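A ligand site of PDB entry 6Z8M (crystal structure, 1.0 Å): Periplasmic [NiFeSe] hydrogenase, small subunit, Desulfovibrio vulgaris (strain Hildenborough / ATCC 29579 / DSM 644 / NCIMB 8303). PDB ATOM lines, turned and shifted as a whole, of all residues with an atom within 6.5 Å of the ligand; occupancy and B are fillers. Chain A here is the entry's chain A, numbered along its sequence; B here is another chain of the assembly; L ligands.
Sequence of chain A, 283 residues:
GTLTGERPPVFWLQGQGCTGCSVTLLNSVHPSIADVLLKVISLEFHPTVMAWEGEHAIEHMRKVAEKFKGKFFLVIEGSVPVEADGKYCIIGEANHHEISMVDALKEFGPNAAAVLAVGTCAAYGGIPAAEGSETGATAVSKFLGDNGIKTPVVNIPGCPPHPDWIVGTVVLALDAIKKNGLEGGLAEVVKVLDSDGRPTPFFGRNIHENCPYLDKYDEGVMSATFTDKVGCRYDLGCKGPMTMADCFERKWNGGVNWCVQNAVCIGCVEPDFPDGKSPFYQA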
ATOM      1  N   GLN A  16     -25.310  18.551 -13.036  1.00  0.00           N
ATOM      2  CA  GLN A  16     -24.026  19.251 -13.007  1.00  0.00           C
ATOM      3  C   GLN A  16     -22.945  18.328 -13.526  1.00  0.00           C
ATOM      4  O   GLN A  16     -22.038  17.903 -12.802  1.00  0.00           O
ATOM      5  CB  GLN A  16     -23.720  19.716 -11.593  1.00  0.00           C
ATOM      6  CG  GLN A  16     -24.639  20.798 -11.077  1.00  0.00           C
ATOM      7  CD  GLN A  16     -24.429  21.031  -9.608  1.00  0.00           C
ATOM      8  OE1 GLN A  16     -24.588  20.120  -8.814  1.00  0.00           O
ATOM      9  NE2 GLN A  16     -24.049  22.255  -9.244  1.00  0.00           N
ATOM     10  N   GLY A  17     -23.039  18.038 -14.826  1.00  0.00           N
ATOM     11  CA  GLY A  17     -22.056  17.253 -15.537  1.00  0.00           C
ATOM     12  C   GLY A  17     -21.251  18.125 -16.479  1.00  0.00           C
ATOM     13  O   GLY A  17     -21.496  19.327 -16.646  1.00  0.00           O
ATOM     14  N   CYS A  18     -20.269  17.499 -17.114  1.00  0.00           N
ATOM     15  CA  CYS A  18     -19.406  18.173 -18.070  1.00  0.00           C
ATOM     16  C   CYS A  18     -19.540  17.597 -19.460  1.00  0.00           C
ATOM     17  O   CYS A  18     -18.807  18.011 -20.367  1.00  0.00           O
ATOM     18  CB  CYS A  18     -17.941  18.111 -17.634  1.00  0.00           C
ATOM     19  SG  CYS A  18     -17.128  16.528 -17.934  1.00  0.00           S
ATOM     20  N   THR A  19     -20.461  16.644 -19.647  1.00  0.00           N
ATOM     21  CA  THR A  19     -20.698  15.931 -20.897  1.00  0.00           C
ATOM     22  C   THR A  19     -19.589  14.917 -21.169  1.00  0.00           C
ATOM     23  O   THR A  19     -19.666  14.153 -22.153  1.00  0.00           O
ATOM     24  CB  THR A  19     -21.018  16.892 -22.049  1.00  0.00           C
ATOM     25  OG1 THR A  19     -22.115  17.707 -21.610  1.00  0.00           O
ATOM     26  CG2 THR A  19     -21.415  16.168 -23.322  1.00  0.00           C
ATOM     27  N   GLY A  20     -18.605  14.810 -20.283  1.00  0.00           N
ATOM     28  CA  GLY A  20     -17.563  13.827 -20.486  1.00  0.00           C
ATOM     29  C   GLY A  20     -18.006  12.394 -20.312  1.00  0.00           C
ATOM     30  O   GLY A  20     -17.391  11.485 -20.880  1.00  0.00           O
ATOM     31  N   CYS A  21     -19.058  12.173 -19.540  1.00  0.00           N
ATOM     32  CA  CYS A  21     -19.568  10.826 -19.415  1.00  0.00           C
ATOM     33  C   CYS A  21     -20.334  10.408 -20.678  1.00  0.00           C
ATOM     34  O   CYS A  21     -20.292   9.239 -21.066  1.00  0.00           O
ATOM     35  CB  CYS A  21     -20.415  10.719 -18.151  1.00  0.00           C
ATOM     36  SG  CYS A  21     -19.498  10.740 -16.559  1.00  0.00           S
ATOM     37  N   SER A  22     -20.998  11.356 -21.359  1.00  0.00           N
ATOM     38  CA  SER A  22     -21.531  11.070 -22.688  1.00  0.00           C
ATOM     39  C   SER A  22     -20.410  10.820 -23.688  1.00  0.00           C
ATOM     40  O   SER A  22     -20.458   9.876 -24.489  1.00  0.00           O
ATOM     41  CB  SER A  22     -22.380  12.241 -23.156  1.00  0.00           C
ATOM     42  OG  SER A  22     -23.608  12.318 -22.457  1.00  0.00           O
ATOM     43  N   GLU A  77     -26.122  11.950 -15.530  1.00  0.00           N
ATOM     44  CA  GLU A  77     -24.747  12.422 -15.684  1.00  0.00           C
ATOM     45  C   GLU A  77     -24.666  13.756 -14.946  1.00  0.00           C
ATOM     46  O   GLU A  77     -25.428  14.678 -15.249  1.00  0.00           O
ATOM     47  CB  GLU A  77     -24.441  12.615 -17.170  1.00  0.00           C
ATOM     48  CG  GLU A  77     -23.152  13.381 -17.506  1.00  0.00           C
ATOM     49  CD  GLU A  77     -22.807  13.395 -18.991  1.00  0.00           C
ATOM     50  OE1 GLU A  77     -23.718  13.259 -19.836  1.00  0.00           O
ATOM     51  OE2 GLU A  77     -21.607  13.565 -19.316  1.00  0.00           O
ATOM     52  N   GLY A  78     -23.777  13.863 -13.970  1.00  0.00           N
ATOM     53  CA  GLY A  78     -23.654  15.055 -13.147  1.00  0.00           C
ATOM     54  C   GLY A  78     -24.370  14.906 -11.803  1.00  0.00           C
ATOM     55  O   GLY A  78     -25.233  14.056 -11.612  1.00  0.00           O
ATOM     56  N   SER A  79     -24.008  15.793 -10.873  1.00  0.00           N
ATOM     57  CA  SER A  79     -24.660  15.859  -9.570  1.00  0.00           C
ATOM     58  C   SER A  79     -25.955  16.663  -9.640  1.00  0.00           C
ATOM     59  O   SER A  79     -26.258  17.320 -10.638  1.00  0.00           O
ATOM     60  CB  SER A  79     -23.701  16.445  -8.539  1.00  0.00           C
ATOM     61  OG  SER A  79     -23.181  17.680  -8.992  1.00  0.00           O
ATOM     62  N   VAL A 118     -24.111   7.613 -13.693  1.00  0.00           N
ATOM     63  CA  VAL A 118     -22.920   7.471 -14.520  1.00  0.00           C
ATOM     64  C   VAL A 118     -21.973   8.601 -14.195  1.00  0.00           C
ATOM     65  O   VAL A 118     -22.348   9.776 -14.288  1.00  0.00           O
ATOM     66  CB  VAL A 118     -23.291   7.434 -16.015  1.00  0.00           C
ATOM     67  CG1 VAL A 118     -22.098   7.416 -16.896  1.00  0.00           C
ATOM     68  CG2 VAL A 118     -24.141   6.191 -16.310  1.00  0.00           C
ATOM     69  N   GLY A 119     -20.755   8.241 -13.819  1.00  0.00           N
ATOM     70  CA  GLY A 119     -19.711   9.181 -13.464  1.00  0.00           C
ATOM     71  C   GLY A 119     -19.686   9.454 -11.979  1.00  0.00           C
ATOM     72  O   GLY A 119     -20.695   9.330 -11.272  1.00  0.00           O
ATOM     73  N   THR A 120     -18.515   9.867 -11.511  1.00  0.00           N
ATOM     74  CA  THR A 120     -18.331  10.175 -10.102  1.00  0.00           C
ATOM     75  C   THR A 120     -19.208  11.327  -9.618  1.00  0.00           C
ATOM     76  O   THR A 120     -19.642  11.301  -8.456  1.00  0.00           O
ATOM     77  CB  THR A 120     -16.847  10.412  -9.869  1.00  0.00           C
ATOM     78  OG1 THR A 120     -16.202   9.157 -10.116  1.00  0.00           O
ATOM     79  CG2 THR A 120     -16.535  10.892  -8.461  1.00  0.00           C
ATOM     80  N   CYS A 121     -19.520  12.311 -10.468  1.00  0.00           N
ATOM     81  CA  CYS A 121     -20.414  13.383 -10.023  1.00  0.00           C
ATOM     82  C   CYS A 121     -21.757  12.818  -9.606  1.00  0.00           C
ATOM     83  O   CYS A 121     -22.257  13.096  -8.508  1.00  0.00           O
ATOM     84  CB  CYS A 121     -20.632  14.428 -11.121  1.00  0.00           C
ATOM     85  SG  CYS A 121     -19.163  15.318 -11.680  1.00  0.00           S
ATOM     86  N   ALA A 122     -22.391  12.068 -10.505  1.00  0.00           N
ATOM     87  CA  ALA A 122     -23.695  11.481 -10.214  1.00  0.00           C
ATOM     88  C   ALA A 122     -23.605  10.467  -9.094  1.00  0.00           C
ATOM     89  O   ALA A 122     -24.474  10.395  -8.222  1.00  0.00           O
ATOM     90  CB  ALA A 122     -24.260  10.847 -11.473  1.00  0.00           C
ATOM     91  N   GLY A 126     -18.662  14.220  -6.530  1.00  0.00           N
ATOM     92  CA  GLY A 126     -17.555  14.572  -7.403  1.00  0.00           C
ATOM     93  C   GLY A 126     -17.099  16.016  -7.248  1.00  0.00           C
ATOM     94  O   GLY A 126     -17.244  16.655  -6.201  1.00  0.00           O
ATOM     95  N   ILE A 127     -16.521  16.532  -8.334  1.00  0.00           N
ATOM     96  CA  ILE A 127     -15.969  17.895  -8.298  1.00  0.00           C
ATOM     97  C   ILE A 127     -17.017  18.937  -7.936  1.00  0.00           C
ATOM     98  O   ILE A 127     -16.715  19.815  -7.117  1.00  0.00           O
ATOM     99  CB  ILE A 127     -15.185  18.184  -9.580  1.00  0.00           C
ATOM    100  CG1 ILE A 127     -13.905  17.327  -9.581  1.00  0.00           C
ATOM    101  CG2 ILE A 127     -14.814  19.662  -9.675  1.00  0.00           C
ATOM    102  CD1 ILE A 127     -13.105  17.335 -10.847  1.00  0.00           C
ATOM    103  N   PRO A 128     -18.255  18.880  -8.434  1.00  0.00           N
ATOM    104  CA  PRO A 128     -19.229  19.911  -8.043  1.00  0.00           C
ATOM    105  C   PRO A 128     -19.544  19.956  -6.564  1.00  0.00           C
ATOM    106  O   PRO A 128     -20.006  20.985  -6.075  1.00  0.00           O
ATOM    107  CB  PRO A 128     -20.475  19.557  -8.876  1.00  0.00           C
ATOM    108  CG  PRO A 128     -19.898  18.874 -10.083  1.00  0.00           C
ATOM    109  CD  PRO A 128     -18.780  18.041  -9.531  1.00  0.00           C
ATOM    110  N   GLY A 158     -16.110   7.001 -12.051  1.00  0.00           N
ATOM    111  CA  GLY A 158     -15.037   7.390 -12.931  1.00  0.00           C
ATOM    112  C   GLY A 158     -15.244   8.813 -13.400  1.00  0.00           C
ATOM    113  O   GLY A 158     -16.379   9.299 -13.451  1.00  0.00           O
ATOM    114  N   CYS A 159     -14.174   9.494 -13.741  1.00  0.00           N
ATOM    115  CA  CYS A 159     -14.250  10.894 -14.152  1.00  0.00           C
ATOM    116  C   CYS A 159     -13.358  11.079 -15.369  1.00  0.00           C
ATOM    117  O   CYS A 159     -12.239  11.618 -15.276  1.00  0.00           O
ATOM    118  CB  CYS A 159     -13.872  11.817 -13.000  1.00  0.00           C
ATOM    119  SG  CYS A 159     -14.285  13.553 -13.284  1.00  0.00           S
ATOM    120  N   PRO A 160     -13.781  10.593 -16.520  1.00  0.00           N
ATOM    121  CA  PRO A 160     -15.019   9.853 -16.737  1.00  0.00           C
ATOM    122  C   PRO A 160     -14.846   8.352 -16.497  1.00  0.00           C
ATOM    123  O   PRO A 160     -13.718   7.852 -16.403  1.00  0.00           O
ATOM    124  CB  PRO A 160     -15.274  10.055 -18.243  1.00  0.00           C
ATOM    125  CG  PRO A 160     -13.882  10.049 -18.806  1.00  0.00           C
ATOM    126  CD  PRO A 160     -13.010  10.742 -17.772  1.00  0.00           C
ATOM    127  N   PRO A 161     -15.941   7.612 -16.452  1.00  0.00           N
ATOM    128  CA  PRO A 161     -15.850   6.156 -16.572  1.00  0.00           C
ATOM    129  C   PRO A 161     -15.251   5.751 -17.906  1.00  0.00           C
ATOM    130  O   PRO A 161     -15.283   6.485 -18.888  1.00  0.00           O
ATOM    131  CB  PRO A 161     -17.310   5.701 -16.479  1.00  0.00           C
ATOM    132  CG  PRO A 161     -18.067   6.895 -15.947  1.00  0.00           C
ATOM    133  CD  PRO A 161     -17.332   8.089 -16.446  1.00  0.00           C
ATOM    134  N   PHE A 273     -13.300  11.303  -4.401  1.00  0.00           N
ATOM    135  CA  PHE A 273     -12.677  12.099  -5.456  1.00  0.00           C
ATOM    136  C   PHE A 273     -13.464  13.403  -5.640  1.00  0.00           C
ATOM    137  O   PHE A 273     -14.685  13.359  -5.779  1.00  0.00           O
ATOM    138  CB  PHE A 273     -12.657  11.317  -6.763  1.00  0.00           C
ATOM    139  CG  PHE A 273     -12.071  12.081  -7.928  1.00  0.00           C
ATOM    140  CD1 PHE A 273     -10.690  12.109  -8.125  1.00  0.00           C
ATOM    141  CD2 PHE A 273     -12.891  12.768  -8.809  1.00  0.00           C
ATOM    142  CE1 PHE A 273     -10.154  12.818  -9.173  1.00  0.00           C
ATOM    143  CE2 PHE A 273     -12.361  13.471  -9.862  1.00  0.00           C
ATOM    144  CZ  PHE A 273     -10.997  13.513 -10.057  1.00  0.00           C
ATOM    145  N   ARG B  42     -21.622  25.388 -11.646  1.00  0.00           N
ATOM    146  CA  ARG B  42     -20.821  24.597 -10.695  1.00  0.00           C
ATOM    147  C   ARG B  42     -19.850  25.424  -9.869  1.00  0.00           C
ATOM    148  O   ARG B  42     -19.655  25.110  -8.693  1.00  0.00           O
ATOM    149  CB  ARG B  42     -20.080  23.488 -11.442  1.00  0.00           C
ATOM    150  CG  ARG B  42     -21.051  22.396 -11.919  1.00  0.00           C
ATOM    151  CD  ARG B  42     -20.512  21.503 -13.025  1.00  0.00           C
ATOM    152  NE  ARG B  42     -20.180  22.302 -14.188  1.00  0.00           N
ATOM    153  CZ  ARG B  42     -19.282  21.959 -15.106  1.00  0.00           C
ATOM    154  NH1 ARG B  42     -18.674  20.788 -15.076  1.00  0.00           N
ATOM    155  NH2 ARG B  42     -18.989  22.815 -16.087  1.00  0.00           N
ATOM    156  N   PHE B  44     -16.348  26.421 -10.584  1.00  0.00           N
ATOM    157  CA  PHE B  44     -14.959  25.978 -10.535  1.00  0.00           C
ATOM    158  C   PHE B  44     -14.037  27.047  -9.960  1.00  0.00           C
ATOM    159  O   PHE B  44     -13.047  26.711  -9.298  1.00  0.00           O
ATOM    160  CB  PHE B  44     -14.474  25.574 -11.919  1.00  0.00           C
ATOM    161  CG  PHE B  44     -14.917  24.204 -12.305  1.00  0.00           C
ATOM    162  CD1 PHE B  44     -16.242  23.931 -12.626  1.00  0.00           C
ATOM    163  CD2 PHE B  44     -14.019  23.144 -12.302  1.00  0.00           C
ATOM    164  CE1 PHE B  44     -16.641  22.658 -12.949  1.00  0.00           C
ATOM    165  CE2 PHE B  44     -14.424  21.884 -12.615  1.00  0.00           C
ATOM    166  CZ  PHE B  44     -15.726  21.627 -12.941  1.00  0.00           C
ATOM    167  N   ARG B  62     -12.565  19.226 -15.935  1.00  0.00           N
ATOM    168  CA  ARG B  62     -13.932  18.821 -15.662  1.00  0.00           C
ATOM    169  C   ARG B  62     -14.928  19.959 -15.842  1.00  0.00           C
ATOM    170  O   ARG B  62     -16.135  19.731 -15.684  1.00  0.00           O
ATOM    171  CB  ARG B  62     -14.038  18.181 -14.288  1.00  0.00           C
ATOM    172  CG  ARG B  62     -13.501  16.746 -14.266  1.00  0.00           C
ATOM    173  CD  ARG B  62     -11.999  16.641 -14.266  1.00  0.00           C
ATOM    174  NE  ARG B  62     -11.623  15.232 -14.236  1.00  0.00           N
ATOM    175  CZ  ARG B  62     -10.405  14.768 -14.449  1.00  0.00           C
ATOM    176  NH1 ARG B  62      -9.381  15.591 -14.610  1.00  0.00           N
ATOM    177  NH2 ARG B  62     -10.223  13.449 -14.489  1.00  0.00           N
ATOM    178  N   ILE B  63     -14.473  21.138 -16.252  1.00  0.00           N
ATOM    179  CA  ILE B  63     -15.407  22.117 -16.778  1.00  0.00           C
ATOM    180  C   ILE B  63     -16.165  21.528 -17.961  1.00  0.00           C
ATOM    181  O   ILE B  63     -17.348  21.784 -18.138  1.00  0.00           O
ATOM    182  CB  ILE B  63     -14.652  23.408 -17.170  1.00  0.00           C
ATOM    183  CG1 ILE B  63     -14.208  24.126 -15.901  1.00  0.00           C
ATOM    184  CG2 ILE B  63     -15.541  24.289 -18.058  1.00  0.00           C
ATOM    185  CD1 ILE B  63     -13.210  25.221 -16.151  1.00  0.00           C
ATOM    186  N   CYS B  64     -15.497  20.690 -18.744  1.00  0.00           N
ATOM    187  CA  CYS B  64     -16.108  20.244 -19.969  1.00  0.00           C
ATOM    188  C   CYS B  64     -15.351  19.050 -20.501  1.00  0.00           C
ATOM    189  O   CYS B  64     -14.133  19.091 -20.656  1.00  0.00           O
ATOM    190  CB  CYS B  64     -16.079  21.342 -21.035  1.00  0.00           C
ATOM    191  SG  CYS B  64     -16.693  20.685 -22.589  1.00  0.00           S
ATOM    192  N   GLY B  65     -16.085  17.985 -20.793  1.00  0.00           N
ATOM    193  CA  GLY B  65     -15.507  16.767 -21.313  1.00  0.00           C
ATOM    194  C   GLY B  65     -15.474  16.662 -22.815  1.00  0.00           C
ATOM    195  O   GLY B  65     -14.982  15.652 -23.342  1.00  0.00           O
ATOM    196  N   PRO B 173     -11.969  11.407 -22.540  1.00  0.00           N
ATOM    197  CA  PRO B 173     -11.823  12.714 -21.896  1.00  0.00           C
ATOM    198  C   PRO B 173     -10.895  12.696 -20.683  1.00  0.00           C
ATOM    199  O   PRO B 173     -10.704  11.684 -20.006  1.00  0.00           O
ATOM    200  CB  PRO B 173     -13.239  13.043 -21.426  1.00  0.00           C
ATOM    201  CG  PRO B 173     -14.126  12.276 -22.356  1.00  0.00           C
ATOM    202  CD  PRO B 173     -13.388  11.007 -22.649  1.00  0.00           C
ATOM    203  N   HIS B 174     -10.326  13.891 -20.445  1.00  0.00           N
ATOM    204  CA  HIS B 174      -9.587  14.277 -19.246  1.00  0.00           C
ATOM    205  C   HIS B 174      -8.185  13.697 -19.236  1.00  0.00           C
ATOM    206  O   HIS B 174      -7.890  12.664 -18.610  1.00  0.00           O
ATOM    207  CB  HIS B 174     -10.383  13.989 -17.973  1.00  0.00           C
ATOM    208  CG  HIS B 174     -11.698  14.680 -17.962  1.00  0.00           C
ATOM    209  ND1 HIS B 174     -11.911  15.877 -18.626  1.00  0.00           N
ATOM    210  CD2 HIS B 174     -12.871  14.341 -17.391  1.00  0.00           C
ATOM    211  CE1 HIS B 174     -13.169  16.232 -18.449  1.00  0.00           C
ATOM    212  NE2 HIS B 174     -13.772  15.328 -17.700  1.00  0.00           N
HETATM  213 FE1  LIG L   1     -17.652  15.152 -16.225  1.00  0.00          FE
HETATM  214 FE2  LIG L   1     -18.664  14.481 -13.746  1.00  0.00          FE
HETATM  215 FE3  LIG L   1     -16.265  13.623 -14.479  1.00  0.00          FE
HETATM  216 FE4  LIG L   1     -18.464  12.589 -15.808  1.00  0.00          FE
HETATM  217  S1  LIG L   1     -17.941  12.311 -13.615  1.00  0.00           S
HETATM  218  S2  LIG L   1     -16.447  13.258 -16.721  1.00  0.00           S
HETATM  219  S3  LIG L   1     -19.835  14.471 -15.720  1.00  0.00           S
HETATM  220  S4  LIG L   1     -16.872  15.832 -14.237  1.00  0.00           S
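SG of Cys 18 is bound to FE1 of the ligand (2.3 Å). N of Cys 121 lies close to S1 of the ligand. SG of Cys 159 binds FE3 of the ligand, at 2.3 Å. The backbone NH (N) of Cys 18 lies close to a sulfur (S3) of the ligand (3.4 Å). An iron atom (FE2) of the ligand is bound by the side-chain sulfur (SG) of Cys 121 (2.3 Å). FE4 of the ligand is bound by SG of Cys 21, at 2.2 Å. A sulfur (S2) of the ligand sits close to a ring nitrogen (NE2) of His 174 of chain B, 3.5 Å away. A sulfur (S1) of the ligand sits close to the backbone NH (N) of Thr 120, 3.3 Å away.
The backbone NH (N) of Gly 20 sits close to the side-chain sulfur (SG) of Cys 18 (3.3 Å). NE2 of His 174 of chain B lies close to SG of Cys 18 (3.6 Å). OG1 of Thr 120 sits at hydrogen-bond distance from N of Gly 158 (2.9 Å). The backbone NH of Gly 65 of chain B sits at hydrogen-bond distance from the backbone carbonyl oxygen of Cys 18, at 2.8 Å. The side-chain carboxylate of Glu 77 sits at hydrogen-bond distance from the side-chain hydroxyl of Ser 22, 2.8 Å away. SG of Cys 21 sits close to O of Val 118 (3.8 Å). O of Cys 159 sits at hydrogen-bond distance from NH2 of Arg 62 of chain B, 2.8 Å away. OE2 of Glu 77 is in hydrogen-bond range of N of Cys 21 (2.9 Å).
The backbone carbonyl oxygen of Gly 158 lies close to a sulfur (S1) of the ligand. The backbone nitrogen (N) of Pro 160 lies close to a sulfur (S2) of the ligand (3.8 Å). Merely in contact with the ligand: Gly 17, Gly 20, Glu 77, Gly 119 and Arg 62 of chain B. Hydrophobic or aromatic side chains within 4 Å of the ligand: Pro 160 and His 174 of chain B. 13 residues have an atom within 4 Å of the ligand: Gly 17, Cys 18, Gly 20, Cys 21, Glu 77, Gly 119, Thr 120, Cys 121, Gly 158, Cys 159, Pro 160, Arg 62 of chain B and His 174 of chain B. The nearest printed residue that does not touch the ligand is Gly 78 (4.4 Å).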
